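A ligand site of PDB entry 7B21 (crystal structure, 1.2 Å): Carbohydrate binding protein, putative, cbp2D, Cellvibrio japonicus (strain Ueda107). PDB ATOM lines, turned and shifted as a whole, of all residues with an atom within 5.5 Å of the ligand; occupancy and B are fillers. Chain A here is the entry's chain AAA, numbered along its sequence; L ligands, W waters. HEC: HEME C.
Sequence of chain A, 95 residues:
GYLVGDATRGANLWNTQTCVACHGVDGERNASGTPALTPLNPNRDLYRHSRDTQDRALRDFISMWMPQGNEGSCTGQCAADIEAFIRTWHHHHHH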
ATOM      1  N   TRP A  14      19.513  -2.198   1.345  1.00  0.00           N
ATOM      2  CA  TRP A  14      20.479  -1.189   1.763  1.00  0.00           C
ATOM      3  C   TRP A  14      19.855   0.191   1.687  1.00  0.00           C
ATOM      4  O   TRP A  14      20.139   1.078   2.522  1.00  0.00           O
ATOM      5  CB  TRP A  14      21.692  -1.307   0.841  1.00  0.00           C
ATOM      6  CG  TRP A  14      22.721  -0.283   1.112  1.00  0.00           C
ATOM      7  CD1 TRP A  14      22.943   0.866   0.420  1.00  0.00           C
ATOM      8  CD2 TRP A  14      23.628  -0.257   2.239  1.00  0.00           C
ATOM      9  NE1 TRP A  14      23.913   1.611   1.039  1.00  0.00           N
ATOM     10  CE2 TRP A  14      24.357   0.924   2.137  1.00  0.00           C
ATOM     11  CE3 TRP A  14      23.904  -1.155   3.275  1.00  0.00           C
ATOM     12  CZ2 TRP A  14      25.299   1.274   3.091  1.00  0.00           C
ATOM     13  CZ3 TRP A  14      24.853  -0.816   4.211  1.00  0.00           C
ATOM     14  CH2 TRP A  14      25.507   0.415   4.141  1.00  0.00           C
ATOM     15  N   GLN A  17      15.970   0.179   3.814  1.00  0.00           N
ATOM     16  CA  GLN A  17      16.144   0.145   5.280  1.00  0.00           C
ATOM     17  C   GLN A  17      16.995   1.294   5.796  1.00  0.00           C
ATOM     18  O   GLN A  17      17.302   1.312   6.979  1.00  0.00           O
ATOM     19  CB  GLN A  17      16.716  -1.197   5.681  1.00  0.00           C
ATOM     20  CG  GLN A  17      15.869  -2.379   5.188  1.00  0.00           C
ATOM     21  CD  GLN A  17      14.356  -2.322   5.319  1.00  0.00           C
ATOM     22  OE1 GLN A  17      13.869  -2.453   6.409  1.00  0.00           O
ATOM     23  NE2 GLN A  17      13.624  -2.079   4.214  1.00  0.00           N
ATOM     24  N   THR A  18      17.325   2.266   4.919  1.00  0.00           N
ATOM     25  CA  THR A  18      17.889   3.568   5.212  1.00  0.00           C
ATOM     26  C   THR A  18      19.382   3.535   5.486  1.00  0.00           C
ATOM     27  O   THR A  18      19.954   4.599   5.789  1.00  0.00           O
ATOM     28  CB  THR A  18      17.165   4.350   6.334  1.00  0.00           C
ATOM     29  OG1 THR A  18      17.564   3.867   7.626  1.00  0.00           O
ATOM     30  CG2 THR A  18      15.674   4.330   6.158  1.00  0.00           C
ATOM     31  N   CYS A  19      20.040   2.393   5.353  1.00  0.00           N
ATOM     32  CA  CYS A  19      21.495   2.291   5.588  1.00  0.00           C
ATOM     33  C   CYS A  19      22.276   3.335   4.790  1.00  0.00           C
ATOM     34  O   CYS A  19      23.226   3.932   5.305  1.00  0.00           O
ATOM     35  CB  CYS A  19      21.993   0.900   5.196  1.00  0.00           C
ATOM     36  SG  CYS A  19      20.912  -0.478   5.619  1.00  0.00           S
ATOM     37  N   ALA A  21      21.609   6.315   4.099  1.00  0.00           N
ATOM     38  CA  ALA A  21      21.660   7.680   4.640  1.00  0.00           C
ATOM     39  C   ALA A  21      22.955   7.887   5.416  1.00  0.00           C
ATOM     40  O   ALA A  21      23.623   8.923   5.258  1.00  0.00           O
ATOM     41  CB  ALA A  21      20.470   7.918   5.521  1.00  0.00           C
ATOM     42  N   CYS A  22      23.320   6.960   6.326  1.00  0.00           N
ATOM     43  CA  CYS A  22      24.457   7.140   7.195  1.00  0.00           C
ATOM     44  C   CYS A  22      25.737   6.600   6.586  1.00  0.00           C
ATOM     45  O   CYS A  22      26.803   7.085   6.940  1.00  0.00           O
ATOM     46  CB  CYS A  22      24.216   6.534   8.544  1.00  0.00           C
ATOM     47  SG  CYS A  22      22.853   7.405   9.377  1.00  0.00           S
ATOM     48  N   HIS A  23      25.642   5.578   5.754  1.00  0.00           N
ATOM     49  CA  HIS A  23      26.824   4.843   5.287  1.00  0.00           C
ATOM     50  C   HIS A  23      27.083   5.034   3.797  1.00  0.00           C
ATOM     51  O   HIS A  23      28.005   4.395   3.268  1.00  0.00           O
ATOM     52  CB  HIS A  23      26.667   3.346   5.611  1.00  0.00           C
ATOM     53  CG  HIS A  23      26.595   3.045   7.069  1.00  0.00           C
ATOM     54  ND1 HIS A  23      27.624   3.330   7.932  1.00  0.00           N
ATOM     55  CD2 HIS A  23      25.676   2.399   7.812  1.00  0.00           C
ATOM     56  CE1 HIS A  23      27.284   2.875   9.130  1.00  0.00           C
ATOM     57  NE2 HIS A  23      26.086   2.277   9.111  1.00  0.00           N
ATOM     58  N   THR A  38      29.137   8.049   8.146  1.00  0.00           N
ATOM     59  CA  THR A  38      29.749   7.023   8.993  1.00  0.00           C
ATOM     60  C   THR A  38      30.301   5.957   8.056  1.00  0.00           C
ATOM     61  O   THR A  38      29.553   5.240   7.387  1.00  0.00           O
ATOM     62  CB  THR A  38      28.730   6.412   9.943  1.00  0.00           C
ATOM     63  OG1 THR A  38      28.190   7.447  10.763  1.00  0.00           O
ATOM     64  CG2 THR A  38      29.354   5.349  10.823  1.00  0.00           C
ATOM     65  N   PRO A  39      31.619   5.804   7.997  1.00  0.00           N
ATOM     66  CA  PRO A  39      32.195   4.760   7.174  1.00  0.00           C
ATOM     67  C   PRO A  39      31.726   3.395   7.634  1.00  0.00           C
ATOM     68  O   PRO A  39      31.364   3.168   8.793  1.00  0.00           O
ATOM     69  CB  PRO A  39      33.700   4.914   7.293  1.00  0.00           C
ATOM     70  CG  PRO A  39      33.943   6.092   8.097  1.00  0.00           C
ATOM     71  CD  PRO A  39      32.654   6.674   8.573  1.00  0.00           C
ATOM     72  N   LEU A  40      31.814   2.443   6.730  1.00  0.00           N
ATOM     73  CA  LEU A  40      31.498   1.027   7.004  1.00  0.00           C
ATOM     74  C   LEU A  40      32.581   0.194   6.345  1.00  0.00           C
ATOM     75  O   LEU A  40      32.698   0.191   5.126  1.00  0.00           O
ATOM     76  CB  LEU A  40      30.112   0.695   6.486  1.00  0.00           C
ATOM     77  CG  LEU A  40      29.468  -0.621   6.942  1.00  0.00           C
ATOM     78  CD1 LEU A  40      28.036  -0.658   6.451  1.00  0.00           C
ATOM     79  CD2 LEU A  40      30.242  -1.860   6.492  1.00  0.00           C
ATOM     80  N   ASN A  41      33.407  -0.456   7.166  1.00  0.00           N
ATOM     81  CA  ASN A  41      34.448  -1.360   6.694  1.00  0.00           C
ATOM     82  C   ASN A  41      33.796  -2.706   6.422  1.00  0.00           C
ATOM     83  O   ASN A  41      33.327  -3.347   7.376  1.00  0.00           O
ATOM     84  CB  ASN A  41      35.527  -1.469   7.737  1.00  0.00           C
ATOM     85  CG  ASN A  41      36.667  -2.348   7.301  1.00  0.00           C
ATOM     86  OD1 ASN A  41      36.507  -3.315   6.558  1.00  0.00           O
ATOM     87  ND2 ASN A  41      37.825  -2.019   7.800  1.00  0.00           N
ATOM     88  N   ARG A  44      35.682  -6.895   7.821  1.00  0.00           N
ATOM     89  CA  ARG A  44      36.026  -7.462   9.144  1.00  0.00           C
ATOM     90  C   ARG A  44      35.451  -8.870   9.210  1.00  0.00           C
ATOM     91  O   ARG A  44      34.377  -9.113   8.678  1.00  0.00           O
ATOM     92  CB  ARG A  44      35.422  -6.665  10.284  1.00  0.00           C
ATOM     93  CG  ARG A  44      35.671  -5.175  10.251  1.00  0.00           C
ATOM     94  CD  ARG A  44      35.281  -4.536  11.549  1.00  0.00           C
ATOM     95  NE  ARG A  44      35.171  -3.115  11.462  1.00  0.00           N
ATOM     96  CZ  ARG A  44      36.171  -2.230  11.433  1.00  0.00           C
ATOM     97  NH1 ARG A  44      37.415  -2.649  11.566  1.00  0.00           N
ATOM     98  NH2 ARG A  44      35.928  -0.959  11.241  1.00  0.00           N
ATOM     99  N   TYR A  47      32.062  -8.253  13.854  1.00  0.00           N
ATOM    100  CA  TYR A  47      31.729  -6.854  14.124  1.00  0.00           C
ATOM    101  C   TYR A  47      31.293  -6.754  15.571  1.00  0.00           C
ATOM    102  O   TYR A  47      30.381  -7.454  16.025  1.00  0.00           O
ATOM    103  CB  TYR A  47      30.628  -6.375  13.175  1.00  0.00           C
ATOM    104  CG  TYR A  47      31.101  -6.242  11.756  1.00  0.00           C
ATOM    105  CD1 TYR A  47      31.195  -7.321  10.915  1.00  0.00           C
ATOM    106  CD2 TYR A  47      31.524  -5.020  11.275  1.00  0.00           C
ATOM    107  CE1 TYR A  47      31.718  -7.202   9.626  1.00  0.00           C
ATOM    108  CE2 TYR A  47      32.024  -4.875  10.010  1.00  0.00           C
ATOM    109  CZ  TYR A  47      32.148  -5.959   9.174  1.00  0.00           C
ATOM    110  OH  TYR A  47      32.703  -5.862   7.936  1.00  0.00           O
ATOM    111  N   ARG A  48      31.908  -5.803  16.282  1.00  0.00           N
ATOM    112  CA  ARG A  48      31.563  -5.543  17.697  1.00  0.00           C
ATOM    113  C   ARG A  48      31.161  -4.084  17.820  1.00  0.00           C
ATOM    114  O   ARG A  48      31.985  -3.195  17.845  1.00  0.00           O
ATOM    115  CB  ARG A  48      32.694  -5.873  18.662  1.00  0.00           C
ATOM    116  CG  ARG A  48      32.252  -5.769  20.116  1.00  0.00           C
ATOM    117  CD  ARG A  48      33.363  -6.206  21.053  1.00  0.00           C
ATOM    118  NE  ARG A  48      33.018  -5.892  22.422  1.00  0.00           N
ATOM    119  CZ  ARG A  48      33.441  -6.515  23.492  1.00  0.00           C
ATOM    120  NH1 ARG A  48      34.261  -7.544  23.405  1.00  0.00           N
ATOM    121  NH2 ARG A  48      33.062  -6.063  24.679  1.00  0.00           N
ATOM    122  N   HIS A  49      29.865  -3.839  17.937  1.00  0.00           N
ATOM    123  CA  HIS A  49      29.336  -2.491  18.186  1.00  0.00           C
ATOM    124  C   HIS A  49      29.978  -1.965  19.460  1.00  0.00           C
ATOM    125  O   HIS A  49      30.239  -2.741  20.410  1.00  0.00           O
ATOM    126  CB  HIS A  49      27.821  -2.566  18.322  1.00  0.00           C
ATOM    127  CG  HIS A  49      27.135  -1.250  18.324  1.00  0.00           C
ATOM    128  ND1 HIS A  49      27.091  -0.447  19.445  1.00  0.00           N
ATOM    129  CD2 HIS A  49      26.451  -0.605  17.346  1.00  0.00           C
ATOM    130  CE1 HIS A  49      26.364   0.634  19.153  1.00  0.00           C
ATOM    131  NE2 HIS A  49      25.970   0.577  17.859  1.00  0.00           N
ATOM    132  N   SER A  50      30.184  -0.664  19.515  1.00  0.00           N
ATOM    133  CA  SER A  50      30.769  -0.028  20.711  1.00  0.00           C
ATOM    134  C   SER A  50      29.979  -0.335  21.987  1.00  0.00           C
ATOM    135  O   SER A  50      30.568  -0.279  23.053  1.00  0.00           O
ATOM    136  CB  SER A  50      30.921   1.442  20.526  1.00  0.00           C
ATOM    137  OG  SER A  50      29.684   2.091  20.387  1.00  0.00           O
ATOM    138  N   ARG A  51      28.703  -0.649  21.898  1.00  0.00           N
ATOM    139  CA  ARG A  51      27.872  -0.946  23.072  1.00  0.00           C
ATOM    140  C   ARG A  51      27.681  -2.436  23.288  1.00  0.00           C
ATOM    141  O   ARG A  51      26.982  -2.822  24.225  1.00  0.00           O
ATOM    142  CB  ARG A  51      26.499  -0.288  22.934  1.00  0.00           C
ATOM    143  CG  ARG A  51      26.510   1.242  22.894  1.00  0.00           C
ATOM    144  CD  ARG A  51      25.060   1.779  22.684  1.00  0.00           C
ATOM    145  NE  ARG A  51      24.016   1.162  23.543  1.00  0.00           N
ATOM    146  CZ  ARG A  51      22.693   1.046  23.289  1.00  0.00           C
ATOM    147  NH1 ARG A  51      22.114   1.594  22.225  1.00  0.00           N
ATOM    148  NH2 ARG A  51      21.919   0.453  24.188  1.00  0.00           N
ATOM    149  N   LEU A  58      28.369 -10.532  10.876  1.00  0.00           N
ATOM    150  CA  LEU A  58      27.841  -9.291  10.287  1.00  0.00           C
ATOM    151  C   LEU A  58      26.305  -9.281  10.303  1.00  0.00           C
ATOM    152  O   LEU A  58      25.694  -8.289  10.687  1.00  0.00           O
ATOM    153  CB  LEU A  58      28.452  -9.106   8.902  1.00  0.00           C
ATOM    154  CG  LEU A  58      27.927  -7.924   8.087  1.00  0.00           C
ATOM    155  CD1 LEU A  58      28.007  -6.616   8.858  1.00  0.00           C
ATOM    156  CD2 LEU A  58      28.726  -7.793   6.821  1.00  0.00           C
ATOM    157  N   PHE A  61      25.124  -8.559  13.803  1.00  0.00           N
ATOM    158  CA  PHE A  61      25.372  -7.134  14.117  1.00  0.00           C
ATOM    159  C   PHE A  61      24.242  -6.299  13.541  1.00  0.00           C
ATOM    160  O   PHE A  61      23.702  -5.422  14.187  1.00  0.00           O
ATOM    161  CB  PHE A  61      26.726  -6.742  13.550  1.00  0.00           C
ATOM    162  CG  PHE A  61      27.026  -5.249  13.705  1.00  0.00           C
ATOM    163  CD1 PHE A  61      26.471  -4.312  12.844  1.00  0.00           C
ATOM    164  CD2 PHE A  61      27.883  -4.812  14.692  1.00  0.00           C
ATOM    165  CE1 PHE A  61      26.748  -2.964  13.005  1.00  0.00           C
ATOM    166  CE2 PHE A  61      28.217  -3.476  14.810  1.00  0.00           C
ATOM    167  CZ  PHE A  61      27.628  -2.554  13.968  1.00  0.00           C
ATOM    168  N   ILE A  62      23.911  -6.556  12.283  1.00  0.00           N
ATOM    169  CA  ILE A  62      22.838  -5.781  11.612  1.00  0.00           C
ATOM    170  C   ILE A  62      21.525  -5.994  12.340  1.00  0.00           C
ATOM    171  O   ILE A  62      20.793  -5.033  12.666  1.00  0.00           O
ATOM    172  CB  ILE A  62      22.752  -6.108  10.123  1.00  0.00           C
ATOM    173  CG1 ILE A  62      24.039  -5.679   9.392  1.00  0.00           C
ATOM    174  CG2 ILE A  62      21.512  -5.504   9.499  1.00  0.00           C
ATOM    175  CD1 ILE A  62      24.169  -6.230   8.002  1.00  0.00           C
ATOM    176  N   MET A  66      21.289  -2.268  13.749  1.00  0.00           N
ATOM    177  CA  MET A  66      21.101  -1.365  12.600  1.00  0.00           C
ATOM    178  C   MET A  66      19.722  -1.577  12.007  1.00  0.00           C
ATOM    179  O   MET A  66      19.147  -2.666  12.057  1.00  0.00           O
ATOM    180  CB  MET A  66      22.185  -1.604  11.562  1.00  0.00           C
ATOM    181  CG  MET A  66      23.590  -1.258  12.061  1.00  0.00           C
ATOM    182  SD  MET A  66      23.864   0.506  12.329  1.00  0.00           S
ATOM    183  CE  MET A  66      24.830   0.448  13.817  1.00  0.00           C
ATOM    184  N   PRO A  67      19.127  -0.563  11.368  1.00  0.00           N
ATOM    185  CA  PRO A  67      19.627   0.818  11.329  1.00  0.00           C
ATOM    186  C   PRO A  67      19.599   1.422  12.725  1.00  0.00           C
ATOM    187  O   PRO A  67      18.672   1.202  13.482  1.00  0.00           O
ATOM    188  CB  PRO A  67      18.648   1.530  10.393  1.00  0.00           C
ATOM    189  CG  PRO A  67      17.339   0.760  10.569  1.00  0.00           C
ATOM    190  CD  PRO A  67      17.796  -0.673  10.773  1.00  0.00           C
ATOM    191  N   GLN A  68      20.610   2.198  13.048  1.00  0.00           N
ATOM    192  CA  GLN A  68      20.711   2.765  14.387  1.00  0.00           C
ATOM    193  C   GLN A  68      19.562   3.768  14.547  1.00  0.00           C
ATOM    194  O   GLN A  68      19.362   4.651  13.722  1.00  0.00           O
ATOM    195  CB  GLN A  68      22.118   3.324  14.558  1.00  0.00           C
ATOM    196  CG  GLN A  68      22.369   3.760  15.982  1.00  0.00           C
ATOM    197  CD  GLN A  68      23.818   3.673  16.414  1.00  0.00           C
ATOM    198  OE1 GLN A  68      24.462   2.603  16.438  1.00  0.00           O
ATOM    199  NE2 GLN A  68      24.347   4.806  16.858  1.00  0.00           N
ATOM    200  N   CYS A  74      15.260  -4.254  10.610  1.00  0.00           N
ATOM    201  CA  CYS A  74      16.036  -5.174   9.739  1.00  0.00           C
ATOM    202  C   CYS A  74      16.612  -6.261  10.610  1.00  0.00           C
ATOM    203  O   CYS A  74      17.545  -5.988  11.385  1.00  0.00           O
ATOM    204  CB  CYS A  74      17.117  -4.456   8.966  1.00  0.00           C
ATOM    205  SG  CYS A  74      18.036  -5.524   7.822  1.00  0.00           S
ATOM    206  N   ILE A  82      21.475  -8.140   3.484  1.00  0.00           N
ATOM    207  CA  ILE A  82      22.381  -6.994   3.461  1.00  0.00           C
ATOM    208  C   ILE A  82      23.808  -7.456   3.800  1.00  0.00           C
ATOM    209  O   ILE A  82      24.744  -6.933   3.194  1.00  0.00           O
ATOM    210  CB  ILE A  82      21.880  -5.866   4.390  1.00  0.00           C
ATOM    211  CG1 ILE A  82      20.537  -5.305   3.915  1.00  0.00           C
ATOM    212  CG2 ILE A  82      22.926  -4.752   4.418  1.00  0.00           C
ATOM    213  CD1 ILE A  82      19.960  -4.228   4.783  1.00  0.00           C
ATOM    214  N   ILE A  86      27.011  -6.413   1.512  1.00  0.00           N
ATOM    215  CA  ILE A  86      28.234  -5.763   2.038  1.00  0.00           C
ATOM    216  C   ILE A  86      29.460  -6.610   1.702  1.00  0.00           C
ATOM    217  O   ILE A  86      30.526  -6.058   1.362  1.00  0.00           O
ATOM    218  CB  ILE A  86      28.088  -5.539   3.542  1.00  0.00           C
ATOM    219  CG1 ILE A  86      27.025  -4.480   3.820  1.00  0.00           C
ATOM    220  CG2 ILE A  86      29.423  -5.151   4.149  1.00  0.00           C
ATOM    221  CD1 ILE A  86      26.633  -4.392   5.260  1.00  0.00           C
HETATM  222 FE   HEC L   1      25.141   1.422  10.612  1.00  0.00          FE
HETATM  223  CHA HEC L   1      28.060   0.913  12.277  1.00  0.00           C
HETATM  224  CHB HEC L   1      25.520  -1.531   9.021  1.00  0.00           C
HETATM  225  CHC HEC L   1      22.104   1.848   9.165  1.00  0.00           C
HETATM  226  CHD HEC L   1      24.943   4.536  11.947  1.00  0.00           C
HETATM  227  NA  HEC L   1      26.506   0.002  10.643  1.00  0.00           N
HETATM  228  C1A HEC L   1      27.709  -0.007  11.317  1.00  0.00           C
HETATM  229  C2A HEC L   1      28.509  -1.125  10.912  1.00  0.00           C
HETATM  230  C3A HEC L   1      27.788  -1.834  10.040  1.00  0.00           C
HETATM  231  C4A HEC L   1      26.536  -1.124   9.850  1.00  0.00           C
HETATM  232  CMA HEC L   1      28.125  -3.139   9.395  1.00  0.00           C
HETATM  233  CAA HEC L   1      29.910  -1.439  11.415  1.00  0.00           C
HETATM  234  CBA HEC L   1      30.967  -0.751  10.516  1.00  0.00           C
HETATM  235  CGA HEC L   1      32.380  -1.075  10.809  1.00  0.00           C
HETATM  236  O1A HEC L   1      32.670  -1.897  11.689  1.00  0.00           O
HETATM  237  O2A HEC L   1      33.257  -0.519  10.068  1.00  0.00           O
HETATM  238  NB  HEC L   1      24.010   0.344   9.351  1.00  0.00           N
HETATM  239  C1B HEC L   1      24.335  -0.860   8.799  1.00  0.00           C
HETATM  240  C2B HEC L   1      23.260  -1.334   7.972  1.00  0.00           C
HETATM  241  C3B HEC L   1      22.258  -0.424   8.044  1.00  0.00           C
HETATM  242  C4B HEC L   1      22.780   0.673   8.893  1.00  0.00           C
HETATM  243  CMB HEC L   1      23.254  -2.607   7.187  1.00  0.00           C
HETATM  244  CAB HEC L   1      20.900  -0.466   7.446  1.00  0.00           C
HETATM  245  CBB HEC L   1      20.079  -1.646   7.882  1.00  0.00           C
HETATM  246  NC  HEC L   1      23.794   2.880  10.563  1.00  0.00           N
HETATM  247  C1C HEC L   1      22.624   2.913   9.881  1.00  0.00           C
HETATM  248  C2C HEC L   1      21.988   4.191   9.979  1.00  0.00           C
HETATM  249  C3C HEC L   1      22.829   4.990  10.696  1.00  0.00           C
HETATM  250  C4C HEC L   1      23.930   4.166  11.100  1.00  0.00           C
HETATM  251  CMC HEC L   1      20.695   4.562   9.293  1.00  0.00           C
HETATM  252  CAC HEC L   1      22.725   6.454  10.985  1.00  0.00           C
HETATM  253  CBC HEC L   1      21.481   6.932  11.621  1.00  0.00           C
HETATM  254  ND  HEC L   1      26.235   2.471  11.926  1.00  0.00           N
HETATM  255  C1D HEC L   1      25.980   3.727  12.382  1.00  0.00           C
HETATM  256  C2D HEC L   1      26.918   4.081  13.429  1.00  0.00           C
HETATM  257  C3D HEC L   1      27.763   3.052  13.583  1.00  0.00           C
HETATM  258  C4D HEC L   1      27.361   2.045  12.579  1.00  0.00           C
HETATM  259  CMD HEC L   1      26.919   5.386  14.174  1.00  0.00           C
HETATM  260  CAD HEC L   1      28.801   2.853  14.628  1.00  0.00           C
HETATM  261  CBD HEC L   1      28.169   1.987  15.796  1.00  0.00           C
HETATM  262  CGD HEC L   1      29.051   1.855  16.999  1.00  0.00           C
HETATM  263  O1D HEC L   1      29.832   0.878  17.098  1.00  0.00           O
HETATM  264  O2D HEC L   1      28.967   2.758  17.885  1.00  0.00           O
HETATM  265  O   HOH W   1      32.002  -2.622  14.241  1.00  0.00           O
HETATM  266  O   HOH W   2      32.689   1.150  17.013  1.00  0.00           O
HETATM  267  O   HOH W   3      34.225   1.989  10.192  1.00  0.00           O
HETATM  268  O   HOH W   4      26.873   4.574  18.074  1.00  0.00           O
HETATM  269  O   HOH W   5      30.347  -0.511  14.827  1.00  0.00           O
HETATM  270  O   HOH W   6      25.685   8.160  11.462  1.00  0.00           O
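The backbone NH (N) of Asn 41 lies within hydrogen-bond range of an oxygen (O2A) of the ligand, 2.9 Å away.
An oxygen (O1D) of the ligand sits at hydrogen-bond distance from the backbone NH of Ser 50 (2.9 Å).
An oxygen (O2D) of the ligand is in hydrogen-bond range of the side-chain hydroxyl (OG) of Ser 50 (2.7 Å).
SG of Cys 22 is covalently linked to CAC of the ligand (1.9 Å).
The side-chain sulfur (SG) of Cys 19 is covalently linked to a carbon (CAB) of the ligand (1.8 Å).
The guanidinium group of Arg 44 is in salt-bridge range of an oxygen (O1A) of the ligand (2.8 Å).
An iron atom (FE) of the ligand is bound by a ring nitrogen (NE2) of His 23 (2.0 Å).
FE of the ligand is bound by SD of Met 66.
ND1 of His 23 is in hydrogen-bond range of O of Thr 38 (2.8 Å).
The backbone carbonyl oxygen of Cys 22 is in hydrogen-bond range of the backbone NH of Thr 38 (2.8 Å).
SD of Met 66 lies close to N of Gln 68, at 3.7 Å.
The side-chain hydroxyl (OH) of Tyr 47 sits at hydrogen-bond distance from the backbone NH (N) of Arg 44, 3.2 Å away.
N of Cys 19 lies within hydrogen-bond range of O of Trp 14, at 3.1 Å.
N of Arg 51 lies within hydrogen-bond range of ND1 of His 49 (2.9 Å).
OE1 of Gln 68 is in hydrogen-bond range of NE2 of His 49, 2.9 Å away.
O of Asn 41 is in hydrogen-bond range of OH of Tyr 47.
Residues that only touch the ligand: Trp 14, Thr 18, Thr 38, Leu 40, Tyr 47, His 49, Leu 58, Phe 61, Ile 62, Pro 67, Gln 68 and Ile 82.
Hydrophobic or aromatic side chains that line the ligand: Trp 14, His 23, Leu 40, Tyr 47, His 49, Leu 58, Phe 61, Ile 62, Met 66, Pro 67 and Ile 82.
The nearest printed residue that does not touch the ligand is Gln 17 (4.04 Å).
Water W3 bridges an oxygen (O2A) of the ligand (2.7 Å) and the backbone carbonyl oxygen (O) of Pro 39 (3.4 Å).
Water W4 bridges an oxygen (O2D) of the ligand and the side-chain amide nitrogen (NE2) of Gln 68.
Water W6 bridges the side-chain hydroxyl (OG1) of Thr 38 (2.7 Å) and the side-chain sulfur (SG) of Cys 22 (3.6 Å).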
